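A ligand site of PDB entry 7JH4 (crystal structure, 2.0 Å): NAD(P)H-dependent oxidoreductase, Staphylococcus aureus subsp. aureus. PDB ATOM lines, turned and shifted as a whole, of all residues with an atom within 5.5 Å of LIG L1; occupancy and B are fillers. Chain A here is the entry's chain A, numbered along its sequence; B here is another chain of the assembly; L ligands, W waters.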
ATOM      1  N   ARG A  15     -30.833   2.034 -11.679  1.00  0.00           N
ATOM      2  CA  ARG A  15     -29.890   3.133 -11.831  1.00  0.00           C
ATOM      3  C   ARG A  15     -29.857   3.994 -10.574  1.00  0.00           C
ATOM      4  O   ARG A  15     -30.905   4.357 -10.032  1.00  0.00           O
ATOM      5  CB  ARG A  15     -30.260   3.993 -13.045  1.00  0.00           C
ATOM      6  CG  ARG A  15     -29.142   4.925 -13.517  1.00  0.00           C
ATOM      7  CD  ARG A  15     -29.672   6.278 -14.003  1.00  0.00           C
ATOM      8  NE  ARG A  15     -30.593   6.835 -13.030  1.00  0.00           N
ATOM      9  CZ  ARG A  15     -30.214   7.476 -11.928  1.00  0.00           C
ATOM     10  NH1 ARG A  15     -31.123   7.923 -11.069  1.00  0.00           N
ATOM     11  NH2 ARG A  15     -28.922   7.675 -11.677  1.00  0.00           N
ATOM     12  N   HIS A  16     -28.656   4.270 -10.091  1.00  0.00           N
ATOM     13  CA  HIS A  16     -28.416   5.283  -9.061  1.00  0.00           C
ATOM     14  C   HIS A  16     -27.064   5.928  -9.368  1.00  0.00           C
ATOM     15  O   HIS A  16     -26.317   5.486 -10.247  1.00  0.00           O
ATOM     16  CB  HIS A  16     -28.418   4.667  -7.660  1.00  0.00           C
ATOM     17  CG  HIS A  16     -27.397   3.593  -7.473  1.00  0.00           C
ATOM     18  ND1 HIS A  16     -27.500   2.356  -8.076  1.00  0.00           N
ATOM     19  CD2 HIS A  16     -26.225   3.578  -6.802  1.00  0.00           C
ATOM     20  CE1 HIS A  16     -26.455   1.620  -7.759  1.00  0.00           C
ATOM     21  NE2 HIS A  16     -25.655   2.338  -6.996  1.00  0.00           N
ATOM     22  N   ALA A  17     -26.742   6.978  -8.615  1.00  0.00           N
ATOM     23  CA  ALA A  17     -25.490   7.721  -8.786  1.00  0.00           C
ATOM     24  C   ALA A  17     -24.364   6.953  -8.108  1.00  0.00           C
ATOM     25  O   ALA A  17     -23.922   7.294  -7.010  1.00  0.00           O
ATOM     26  CB  ALA A  17     -25.615   9.132  -8.223  1.00  0.00           C
ATOM     27  N   LYS A  19     -20.997   5.821  -6.871  1.00  0.00           N
ATOM     28  CA  LYS A  19     -19.681   6.400  -6.631  1.00  0.00           C
ATOM     29  C   LYS A  19     -18.581   5.350  -6.794  1.00  0.00           C
ATOM     30  O   LYS A  19     -17.572   5.593  -7.469  1.00  0.00           O
ATOM     31  CB  LYS A  19     -19.610   6.992  -5.225  1.00  0.00           C
ATOM     32  CG  LYS A  19     -20.929   7.552  -4.710  1.00  0.00           C
ATOM     33  CD  LYS A  19     -21.099   9.007  -5.087  1.00  0.00           C
ATOM     34  CE  LYS A  19     -22.501   9.512  -4.760  1.00  0.00           C
ATOM     35  NZ  LYS A  19     -23.258   9.922  -6.005  1.00  0.00           N
ATOM     36  N   GLY A  71     -16.045  15.771  -7.245  1.00  0.00           N
ATOM     37  CA  GLY A  71     -17.252  14.940  -7.286  1.00  0.00           C
ATOM     38  C   GLY A  71     -17.119  13.660  -8.066  1.00  0.00           C
ATOM     39  O   GLY A  71     -18.050  12.836  -8.068  1.00  0.00           O
ATOM     40  N   ALA A  72     -15.988  13.451  -8.731  1.00  0.00           N
ATOM     41  CA  ALA A  72     -15.785  12.299  -9.597  1.00  0.00           C
ATOM     42  C   ALA A  72     -14.682  11.355  -9.129  1.00  0.00           C
ATOM     43  O   ALA A  72     -14.421  10.371  -9.813  1.00  0.00           O
ATOM     44  CB  ALA A  72     -15.481  12.776 -11.029  1.00  0.00           C
ATOM     45  N   GLN A  75     -15.289   7.587  -8.808  1.00  0.00           N
ATOM     46  CA  GLN A  75     -15.724   7.080 -10.119  1.00  0.00           C
ATOM     47  C   GLN A  75     -14.560   6.981 -11.089  1.00  0.00           C
ATOM     48  O   GLN A  75     -14.433   5.998 -11.835  1.00  0.00           O
ATOM     49  CB  GLN A  75     -16.823   7.970 -10.689  1.00  0.00           C
ATOM     50  CG  GLN A  75     -18.070   8.031  -9.813  1.00  0.00           C
ATOM     51  CD  GLN A  75     -18.046   9.183  -8.812  1.00  0.00           C
ATOM     52  OE1 GLN A  75     -16.981   9.559  -8.287  1.00  0.00           O
ATOM     53  NE2 GLN A  75     -19.223   9.754  -8.547  1.00  0.00           N
ATOM     54  N   TYR A 145     -27.245  16.616 -22.547  1.00  0.00           N
ATOM     55  CA  TYR A 145     -27.878  15.967 -21.405  1.00  0.00           C
ATOM     56  C   TYR A 145     -28.960  15.005 -21.845  1.00  0.00           C
ATOM     57  O   TYR A 145     -29.328  14.111 -21.084  1.00  0.00           O
ATOM     58  CB  TYR A 145     -28.445  17.031 -20.427  1.00  0.00           C
ATOM     59  CG  TYR A 145     -27.398  17.669 -19.523  1.00  0.00           C
ATOM     60  CD1 TYR A 145     -26.298  18.339 -20.069  1.00  0.00           C
ATOM     61  CD2 TYR A 145     -27.500  17.600 -18.134  1.00  0.00           C
ATOM     62  CE1 TYR A 145     -25.337  18.919 -19.250  1.00  0.00           C
ATOM     63  CE2 TYR A 145     -26.536  18.184 -17.306  1.00  0.00           C
ATOM     64  CZ  TYR A 145     -25.456  18.850 -17.878  1.00  0.00           C
ATOM     65  OH  TYR A 145     -24.494  19.433 -17.083  1.00  0.00           O
ATOM     66  N   LEU A 148     -26.818  12.090 -22.369  1.00  0.00           N
ATOM     67  CA  LEU A 148     -26.422  11.629 -21.039  1.00  0.00           C
ATOM     68  C   LEU A 148     -27.498  10.741 -20.408  1.00  0.00           C
ATOM     69  O   LEU A 148     -27.220   9.620 -19.968  1.00  0.00           O
ATOM     70  CB  LEU A 148     -26.111  12.832 -20.145  1.00  0.00           C
ATOM     71  CG  LEU A 148     -25.837  12.529 -18.678  1.00  0.00           C
ATOM     72  CD1 LEU A 148     -24.519  11.750 -18.469  1.00  0.00           C
ATOM     73  CD2 LEU A 148     -25.842  13.784 -17.836  1.00  0.00           C
ATOM     74  N   MET A 152     -27.153   6.547 -19.670  1.00  0.00           N
ATOM     75  CA  MET A 152     -27.321   5.921 -18.362  1.00  0.00           C
ATOM     76  C   MET A 152     -28.494   4.949 -18.364  1.00  0.00           C
ATOM     77  O   MET A 152     -28.400   3.853 -17.790  1.00  0.00           O
ATOM     78  CB  MET A 152     -27.524   7.015 -17.302  1.00  0.00           C
ATOM     79  CG  MET A 152     -26.303   7.880 -17.066  1.00  0.00           C
ATOM     80  SD  MET A 152     -26.595   9.052 -15.742  1.00  0.00           S
ATOM     81  CE  MET A 152     -27.897  10.083 -16.447  1.00  0.00           C
ATOM     82  N   CYS A 163     -22.913   6.818 -13.397  1.00  0.00           N
ATOM     83  CA  CYS A 163     -22.887   7.970 -12.532  1.00  0.00           C
ATOM     84  C   CYS A 163     -22.654   9.216 -13.392  1.00  0.00           C
ATOM     85  O   CYS A 163     -21.652   9.267 -14.107  1.00  0.00           O
ATOM     86  CB  CYS A 163     -21.809   7.873 -11.471  1.00  0.00           C
ATOM     87  SG  CYS A 163     -22.232   9.201 -10.175  1.00  0.00           S
ATOM     88  N   PRO A 164     -23.571  10.189 -13.420  1.00  0.00           N
ATOM     89  CA  PRO A 164     -23.291  11.458 -14.089  1.00  0.00           C
ATOM     90  C   PRO A 164     -22.586  12.388 -13.118  1.00  0.00           C
ATOM     91  O   PRO A 164     -22.769  12.322 -11.908  1.00  0.00           O
ATOM     92  CB  PRO A 164     -24.693  11.967 -14.463  1.00  0.00           C
ATOM     93  CG  PRO A 164     -25.618  11.424 -13.369  1.00  0.00           C
ATOM     94  CD  PRO A 164     -24.901  10.198 -12.756  1.00  0.00           C
ATOM     95  N   MET A 165     -21.712  13.259 -13.659  1.00  0.00           N
ATOM     96  CA  MET A 165     -20.841  14.062 -12.808  1.00  0.00           C
ATOM     97  C   MET A 165     -20.697  15.467 -13.359  1.00  0.00           C
ATOM     98  O   MET A 165     -20.223  15.659 -14.484  1.00  0.00           O
ATOM     99  CB  MET A 165     -19.456  13.418 -12.664  1.00  0.00           C
ATOM    100  CG  MET A 165     -19.426  12.262 -11.696  1.00  0.00           C
ATOM    101  SD  MET A 165     -18.231  10.990 -12.131  1.00  0.00           S
ATOM    102  CE  MET A 165     -18.831  10.536 -13.753  1.00  0.00           C
ATOM    103  N   GLU A 166     -21.094  16.458 -12.547  1.00  0.00           N
ATOM    104  CA  GLU A 166     -20.768  17.853 -12.776  1.00  0.00           C
ATOM    105  C   GLU A 166     -19.719  18.361 -11.796  1.00  0.00           C
ATOM    106  O   GLU A 166     -19.205  19.469 -11.981  1.00  0.00           O
ATOM    107  CB  GLU A 166     -22.012  18.760 -12.668  1.00  0.00           C
ATOM    108  CG  GLU A 166     -22.893  18.789 -13.905  1.00  0.00           C
ATOM    109  CD  GLU A 166     -24.272  19.408 -13.656  1.00  0.00           C
ATOM    110  OE1 GLU A 166     -24.578  19.810 -12.507  1.00  0.00           O
ATOM    111  OE2 GLU A 166     -25.061  19.488 -14.627  1.00  0.00           O
ATOM    112  N   GLY A 167     -19.347  17.550 -10.805  1.00  0.00           N
ATOM    113  CA  GLY A 167     -18.518  17.992  -9.697  1.00  0.00           C
ATOM    114  C   GLY A 167     -17.039  18.098 -10.026  1.00  0.00           C
ATOM    115  O   GLY A 167     -16.219  17.401  -9.421  1.00  0.00           O
ATOM    116  N   PHE A 168     -16.676  18.942 -10.967  1.00  0.00           N
ATOM    117  CA  PHE A 168     -15.265  19.141 -11.281  1.00  0.00           C
ATOM    118  C   PHE A 168     -14.999  20.626 -11.474  1.00  0.00           C
ATOM    119  O   PHE A 168     -15.910  21.429 -11.691  1.00  0.00           O
ATOM    120  CB  PHE A 168     -14.817  18.316 -12.517  1.00  0.00           C
ATOM    121  CG  PHE A 168     -15.700  18.467 -13.750  1.00  0.00           C
ATOM    122  CD1 PHE A 168     -16.821  17.681 -13.914  1.00  0.00           C
ATOM    123  CD2 PHE A 168     -15.372  19.381 -14.744  1.00  0.00           C
ATOM    124  CE1 PHE A 168     -17.614  17.809 -15.040  1.00  0.00           C
ATOM    125  CE2 PHE A 168     -16.156  19.511 -15.873  1.00  0.00           C
ATOM    126  CZ  PHE A 168     -17.293  18.725 -16.022  1.00  0.00           C
ATOM    127  N   VAL A 192     -20.216  17.646 -19.458  1.00  0.00           N
ATOM    128  CA  VAL A 192     -20.570  16.800 -18.327  1.00  0.00           C
ATOM    129  C   VAL A 192     -19.799  15.493 -18.462  1.00  0.00           C
ATOM    130  O   VAL A 192     -19.368  15.117 -19.558  1.00  0.00           O
ATOM    131  CB  VAL A 192     -22.109  16.575 -18.302  1.00  0.00           C
ATOM    132  CG1 VAL A 192     -22.605  15.790 -19.555  1.00  0.00           C
ATOM    133  CG2 VAL A 192     -22.546  15.841 -17.013  1.00  0.00           C
ATOM    134  N   LYS A 207     -33.682   5.305  -2.901  1.00  0.00           N
ATOM    135  CA  LYS A 207     -33.915   6.405  -3.830  1.00  0.00           C
ATOM    136  C   LYS A 207     -35.005   7.298  -3.277  1.00  0.00           C
ATOM    137  O   LYS A 207     -36.022   6.817  -2.780  1.00  0.00           O
ATOM    138  CB  LYS A 207     -34.304   5.856  -5.215  1.00  0.00           C
ATOM    139  CG  LYS A 207     -34.170   6.871  -6.342  1.00  0.00           C
ATOM    140  CD  LYS A 207     -34.605   6.312  -7.710  1.00  0.00           C
ATOM    141  CE  LYS A 207     -33.634   5.284  -8.249  1.00  0.00           C
ATOM    142  NZ  LYS A 207     -32.218   5.664  -7.943  1.00  0.00           N
ATOM    143  N   THR A 208     -34.778   8.616  -3.297  1.00  0.00           N
ATOM    144  CA  THR A 208     -35.794   9.581  -2.909  1.00  0.00           C
ATOM    145  C   THR A 208     -36.120  10.448  -4.117  1.00  0.00           C
ATOM    146  O   THR A 208     -35.216  10.853  -4.864  1.00  0.00           O
ATOM    147  CB  THR A 208     -35.389  10.499  -1.730  1.00  0.00           C
ATOM    148  OG1 THR A 208     -34.050  10.999  -1.926  1.00  0.00           O
ATOM    149  CG2 THR A 208     -35.483   9.773  -0.401  1.00  0.00           C
ATOM    150  N   ARG A 209     -37.406  10.729  -4.292  1.00  0.00           N
ATOM    151  CA  ARG A 209     -37.882  11.670  -5.284  1.00  0.00           C
ATOM    152  C   ARG A 209     -39.094  12.379  -4.695  1.00  0.00           C
ATOM    153  O   ARG A 209     -39.705  11.922  -3.732  1.00  0.00           O
ATOM    154  CB  ARG A 209     -38.241  10.985  -6.610  1.00  0.00           C
ATOM    155  CG  ARG A 209     -37.050  10.365  -7.344  1.00  0.00           C
ATOM    156  CD  ARG A 209     -36.150  11.442  -7.958  1.00  0.00           C
ATOM    157  NE  ARG A 209     -35.152  10.856  -8.863  1.00  0.00           N
ATOM    158  CZ  ARG A 209     -34.022  10.273  -8.467  1.00  0.00           C
ATOM    159  NH1 ARG A 209     -33.177   9.762  -9.358  1.00  0.00           N
ATOM    160  NH2 ARG A 209     -33.707  10.212  -7.182  1.00  0.00           N
ATOM    161  N   LEU B  41     -38.350   9.861 -12.061  1.00  0.00           N
ATOM    162  CA  LEU B  41     -37.238   9.106 -11.497  1.00  0.00           C
ATOM    163  C   LEU B  41     -35.902   9.444 -12.152  1.00  0.00           C
ATOM    164  O   LEU B  41     -34.904   8.773 -11.893  1.00  0.00           O
ATOM    165  CB  LEU B  41     -37.504   7.605 -11.623  1.00  0.00           C
ATOM    166  CG  LEU B  41     -38.811   7.134 -10.965  1.00  0.00           C
ATOM    167  CD1 LEU B  41     -39.161   5.716 -11.428  1.00  0.00           C
ATOM    168  CD2 LEU B  41     -38.699   7.198  -9.459  1.00  0.00           C
ATOM    169  N   PRO B  43     -32.373  11.142 -12.812  1.00  0.00           N
ATOM    170  CA  PRO B  43     -31.382  11.754 -11.926  1.00  0.00           C
ATOM    171  C   PRO B  43     -31.298  13.243 -12.191  1.00  0.00           C
ATOM    172  O   PRO B  43     -31.701  13.725 -13.245  1.00  0.00           O
ATOM    173  CB  PRO B  43     -30.093  11.035 -12.320  1.00  0.00           C
ATOM    174  CG  PRO B  43     -30.260  10.746 -13.781  1.00  0.00           C
ATOM    175  CD  PRO B  43     -31.749  10.367 -13.908  1.00  0.00           C
ATOM    176  N   SER B  44     -30.765  13.975 -11.208  1.00  0.00           N
ATOM    177  CA  SER B  44     -30.555  15.406 -11.407  1.00  0.00           C
ATOM    178  C   SER B  44     -29.348  15.819 -10.579  1.00  0.00           C
ATOM    179  O   SER B  44     -29.028  15.184  -9.569  1.00  0.00           O
ATOM    180  CB  SER B  44     -31.752  16.252 -10.959  1.00  0.00           C
ATOM    181  OG  SER B  44     -32.173  15.812  -9.665  1.00  0.00           O
ATOM    182  N   SER B  45     -28.690  16.899 -10.999  1.00  0.00           N
ATOM    183  CA  SER B  45     -27.496  17.342 -10.303  1.00  0.00           C
ATOM    184  C   SER B  45     -27.887  17.716  -8.881  1.00  0.00           C
ATOM    185  O   SER B  45     -28.889  18.409  -8.663  1.00  0.00           O
ATOM    186  CB  SER B  45     -26.845  18.521 -11.023  1.00  0.00           C
ATOM    187  OG  SER B  45     -25.804  19.118 -10.269  1.00  0.00           O
ATOM    188  N   LEU B  46     -27.144  17.219  -7.888  1.00  0.00           N
ATOM    189  CA  LEU B  46     -27.441  17.403  -6.468  1.00  0.00           C
ATOM    190  C   LEU B  46     -28.794  16.816  -6.051  1.00  0.00           C
ATOM    191  O   LEU B  46     -29.268  17.089  -4.955  1.00  0.00           O
ATOM    192  CB  LEU B  46     -27.376  18.887  -6.083  1.00  0.00           C
ATOM    193  CG  LEU B  46     -26.054  19.632  -6.355  1.00  0.00           C
ATOM    194  CD1 LEU B  46     -26.149  21.108  -5.964  1.00  0.00           C
ATOM    195  CD2 LEU B  46     -24.880  18.984  -5.629  1.00  0.00           C
ATOM    196  N   GLY B  47     -29.445  16.026  -6.918  1.00  0.00           N
ATOM    197  CA  GLY B  47     -30.732  15.450  -6.604  1.00  0.00           C
ATOM    198  C   GLY B  47     -31.866  16.445  -6.476  1.00  0.00           C
ATOM    199  O   GLY B  47     -32.894  16.146  -5.850  1.00  0.00           O
ATOM    200  N   LYS B 106     -34.732  14.856   0.760  1.00  0.00           N
ATOM    201  CA  LYS B 106     -33.485  14.137   0.987  1.00  0.00           C
ATOM    202  C   LYS B 106     -33.209  13.880   2.457  1.00  0.00           C
ATOM    203  O   LYS B 106     -32.359  13.047   2.784  1.00  0.00           O
ATOM    204  CB  LYS B 106     -32.308  14.904   0.354  1.00  0.00           C
ATOM    205  CG  LYS B 106     -32.478  15.232  -1.143  1.00  0.00           C
ATOM    206  CD  LYS B 106     -33.031  14.043  -1.948  1.00  0.00           C
ATOM    207  CE  LYS B 106     -32.216  13.764  -3.211  1.00  0.00           C
ATOM    208  NZ  LYS B 106     -32.490  12.417  -3.807  1.00  0.00           N
ATOM    209  N   GLN B 143     -30.875  19.903 -16.643  1.00  0.00           N
ATOM    210  CA  GLN B 143     -31.362  18.700 -15.962  1.00  0.00           C
ATOM    211  C   GLN B 143     -32.663  18.206 -16.570  1.00  0.00           C
ATOM    212  O   GLN B 143     -32.887  16.986 -16.659  1.00  0.00           O
ATOM    213  CB  GLN B 143     -31.545  18.960 -14.463  1.00  0.00           C
ATOM    214  CG  GLN B 143     -30.450  19.786 -13.811  1.00  0.00           C
ATOM    215  CD  GLN B 143     -29.066  19.177 -13.931  1.00  0.00           C
ATOM    216  OE1 GLN B 143     -28.873  17.970 -13.699  1.00  0.00           O
ATOM    217  NE2 GLN B 143     -28.076  20.017 -14.246  1.00  0.00           N
ATOM    218  N   ILE B 146     -32.341  15.695 -19.361  1.00  0.00           N
ATOM    219  CA  ILE B 146     -32.205  14.292 -18.961  1.00  0.00           C
ATOM    220  C   ILE B 146     -33.581  13.642 -18.916  1.00  0.00           C
ATOM    221  O   ILE B 146     -33.814  12.592 -19.526  1.00  0.00           O
ATOM    222  CB  ILE B 146     -31.487  14.170 -17.602  1.00  0.00           C
ATOM    223  CG1 ILE B 146     -30.089  14.802 -17.657  1.00  0.00           C
ATOM    224  CG2 ILE B 146     -31.409  12.693 -17.165  1.00  0.00           C
ATOM    225  CD1 ILE B 146     -29.444  15.018 -16.273  1.00  0.00           C
HETATM  226  C1  LIG L   1     -25.115  14.381 -10.744  1.00  0.00           C
HETATM  227  N1  LIG L   1     -24.817  13.757  -9.474  1.00  0.00           N
HETATM  228  C2  LIG L   1     -23.441  13.666  -9.079  1.00  0.00           C
HETATM  229  N2  LIG L   1     -23.021  12.632  -8.110  1.00  0.00           N
HETATM  230  C3  LIG L   1     -21.654  12.526  -7.717  1.00  0.00           C
HETATM  231  O1  LIG L   1     -21.292  11.538  -6.818  1.00  0.00           O
HETATM  232  N3  LIG L   1     -20.718  13.433  -8.248  1.00  0.00           N
HETATM  233  C4  LIG L   1     -21.119  14.425  -9.160  1.00  0.00           C
HETATM  234  O2  LIG L   1     -20.186  15.312  -9.681  1.00  0.00           O
HETATM  235  C5  LIG L   1     -22.569  14.517  -9.578  1.00  0.00           C
HETATM  236  N4  LIG L   1     -23.026  15.485 -10.507  1.00  0.00           N
HETATM  237  C6  LIG L   1     -24.261  15.212 -11.217  1.00  0.00           C
HETATM  238  C7  LIG L   1     -24.538  15.889 -12.517  1.00  0.00           C
HETATM  239  C8  LIG L   1     -25.717  15.640 -13.209  1.00  0.00           C
HETATM  240  C9  LIG L   1     -25.945  16.373 -14.524  1.00  0.00           C
HETATM  241  C10 LIG L   1     -26.677  14.735 -12.683  1.00  0.00           C
HETATM  242  C11 LIG L   1     -27.968  14.453 -13.429  1.00  0.00           C
HETATM  243  C12 LIG L   1     -26.403  14.103 -11.481  1.00  0.00           C
HETATM  244  C13 LIG L   1     -25.677  12.682  -9.064  1.00  0.00           C
HETATM  245  C14 LIG L   1     -26.837  13.176  -8.206  1.00  0.00           C
HETATM  246  O3  LIG L   1     -26.437  13.456  -6.912  1.00  0.00           O
HETATM  247  C15 LIG L   1     -27.745  11.959  -8.251  1.00  0.00           C
HETATM  248  O4  LIG L   1     -28.278  11.632  -9.520  1.00  0.00           O
HETATM  249  C16 LIG L   1     -28.916  12.305  -7.362  1.00  0.00           C
HETATM  250  O5  LIG L   1     -28.652  13.038  -6.197  1.00  0.00           O
HETATM  251  C17 LIG L   1     -29.464  11.080  -6.654  1.00  0.00           C
HETATM  252  O6  LIG L   1     -30.396  10.431  -7.407  1.00  0.00           O
HETATM  253  P1  LIG L   1     -29.972   8.941  -7.947  1.00  0.00           P
HETATM  254  O7  LIG L   1     -29.242   9.094  -9.221  1.00  0.00           O
HETATM  255  O8  LIG L   1     -31.195   8.156  -8.172  1.00  0.00           O
HETATM  256  O9  LIG L   1     -29.119   8.112  -7.104  1.00  0.00           O
HETATM  257  N1  LG2 L   2     -20.651  16.809  -6.291  1.00  0.00           N
HETATM  258  C1  LG2 L   2     -21.806  16.099  -6.049  1.00  0.00           C
HETATM  259  C2  LG2 L   2     -22.977  16.360  -6.781  1.00  0.00           C
HETATM  260  C3  LG2 L   2     -24.221  15.563  -6.476  1.00  0.00           C
HETATM  261  O1  LG2 L   2     -25.111  15.511  -7.304  1.00  0.00           O
HETATM  262  N2  LG2 L   2     -24.317  14.865  -5.192  1.00  0.00           N
HETATM  263  C4  LG2 L   2     -22.993  17.327  -7.729  1.00  0.00           C
HETATM  264  C5  LG2 L   2     -21.847  18.048  -7.961  1.00  0.00           C
HETATM  265  C6  LG2 L   2     -20.676  17.775  -7.236  1.00  0.00           C
HETATM  266  O   HOH W   1     -32.015   9.422  -4.611  1.00  0.00           O
HETATM  267  O   HOH W   2     -25.510  11.581  -5.015  1.00  0.00           O
HETATM  268  O   HOH W   3     -27.740   9.109  -4.897  1.00  0.00           O
HETATM  269  O   HOH W   4     -27.106  14.238  -4.014  1.00  0.00           O
HETATM  270  O   HOH W   5     -29.933  11.578  -3.818  1.00  0.00           O
HETATM  271  O   HOH W   6     -30.790   6.842  -5.399  1.00  0.00           O
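The backbone NH (N) of Gly 167 lies within hydrogen-bond range of an oxygen (O2) of LIG L1 (2.6 Å). The side-chain amino group (NZ) of Lys 19 is in hydrogen-bond range of an oxygen (O1) of LIG L1 (2.7 Å). O8 of LIG L1 is in salt-bridge range of NZ of Lys 207, at 2.7 Å. O of Gly 71 is in hydrogen-bond range of N3 of LIG L1, 2.7 Å away. The guanidinium group (NH1) of Arg 209 lies within salt-bridge range of an oxygen (O8) of LIG L1 (2.8 Å). The guanidinium group of Arg 15 is in salt-bridge range of an oxygen (O7) of LIG L1 (2.9 Å). The backbone NH (N) of Glu 166 sits at hydrogen-bond distance from an oxygen (O2) of LIG L1 (3.2 Å). The backbone NH of Ala 17 is in hydrogen-bond range of an oxygen (O9) of LIG L1 (3.0 Å). O5 of LIG L1 is in hydrogen-bond range of N of Gly 47 of chain B, at 3.2 Å. A nitrogen (N4) of LIG L1 lies close to the backbone carbonyl oxygen (O) of Pro 164 (3.5 Å). NE2 of Gln 75 sits at hydrogen-bond distance from O1 of LIG L1 (3.2 Å). The backbone NH (N) of Leu 46 of chain B lies within hydrogen-bond range of an oxygen (O1) of LG2 L2 (2.7 Å).
O3 of LIG L1 lies within hydrogen-bond range of O1 of LG2 L2, 2.5 Å away.
The backbone NH (N) of Gly 71 lies within hydrogen-bond range of the backbone carbonyl oxygen (O) of Gly 167, at 2.7 Å. NZ of Lys 19 is in hydrogen-bond range of O of Ala 17, 2.9 Å away. O of Lys 19 lies within hydrogen-bond range of N of Gln 75, at 3.3 Å. The side-chain amino group (NZ) of Lys 207 is in hydrogen-bond range of the backbone carbonyl oxygen (O) of Arg 15, at 2.8 Å. The backbone carbonyl oxygen (O) of Leu 41 of chain B lies within hydrogen-bond range of the guanidinium group (NH1) of Arg 209, at 3.2 Å. OE2 of Glu 166 sits at hydrogen-bond distance from NE2 of Gln 143 of chain B (3.1 Å). NE2 of Gln 75 sits at hydrogen-bond distance from SG of Cys 163, at 3.5 Å. The side-chain amide oxygen (OE1) of Gln 75 sits close to the backbone carbonyl oxygen (O) of Ala 72, 3.1 Å away.
CA of His 16 touches O9 of LIG L1, at 3.5 Å. Tyr 145 touches LIG L1 (CE2 to C9, 3.4 Å). Met 165 touches LIG L1. Pro 43 of chain B touches LIG L1. O of Ser 44 of chain B touches C14 of LIG L1 (3.3 Å). N of Ser 45 of chain B touches C10 of LIG L1, 3.4 Å away. C of Leu 46 of chain B touches O5 of LIG L1, at 3.8 Å. OE1 of Gln 143 of chain B touches C9 of LIG L1, 3.4 Å away. Ile 146 of chain B touches LIG L1. Hydrophobic or aromatic side chains within 4 Å of LIG L1: His 16, Ala 17, Tyr 145, Pro 164, Met 165, Pro 43 of chain B and Ile 146 of chain B. 20 residues have an atom within 4 Å of LIG L1: Arg 15, His 16, Ala 17, Lys 19, Gly 71, Gln 75, Tyr 145, Pro 164, Met 165, Glu 166, Gly 167, Lys 207, Arg 209, Pro 43 of chain B, Ser 44 of chain B, Ser 45 of chain B, Leu 46 of chain B, Gly 47 of chain B, Gln 143 of chain B and Ile 146 of chain B. Along chain A the residues within 4 Å of LIG L1 span positions 15 to 209. The nearest printed residue that does not touch LIG L1 is Cys 163 (4.1 Å).
Water W6 lies within hydrogen-bond range of O9 of LIG L1 (2.7 Å) and NZ of Lys 207 (3.1 Å). Water W2 lies within hydrogen-bond range of an oxygen (O3) of LIG L1, the side-chain amino group (NZ) of Lys 19 and a nitrogen (N2) of LG2 L2. Water W5 lies within hydrogen-bond range of NZ of Lys 106 of chain B (2.7 Å) and O5 of LIG L1 (3.1 Å). Water W4 bridges O5 of LIG L1 (2.9 Å) and N2 of LG2 L2 (3.1 Å).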
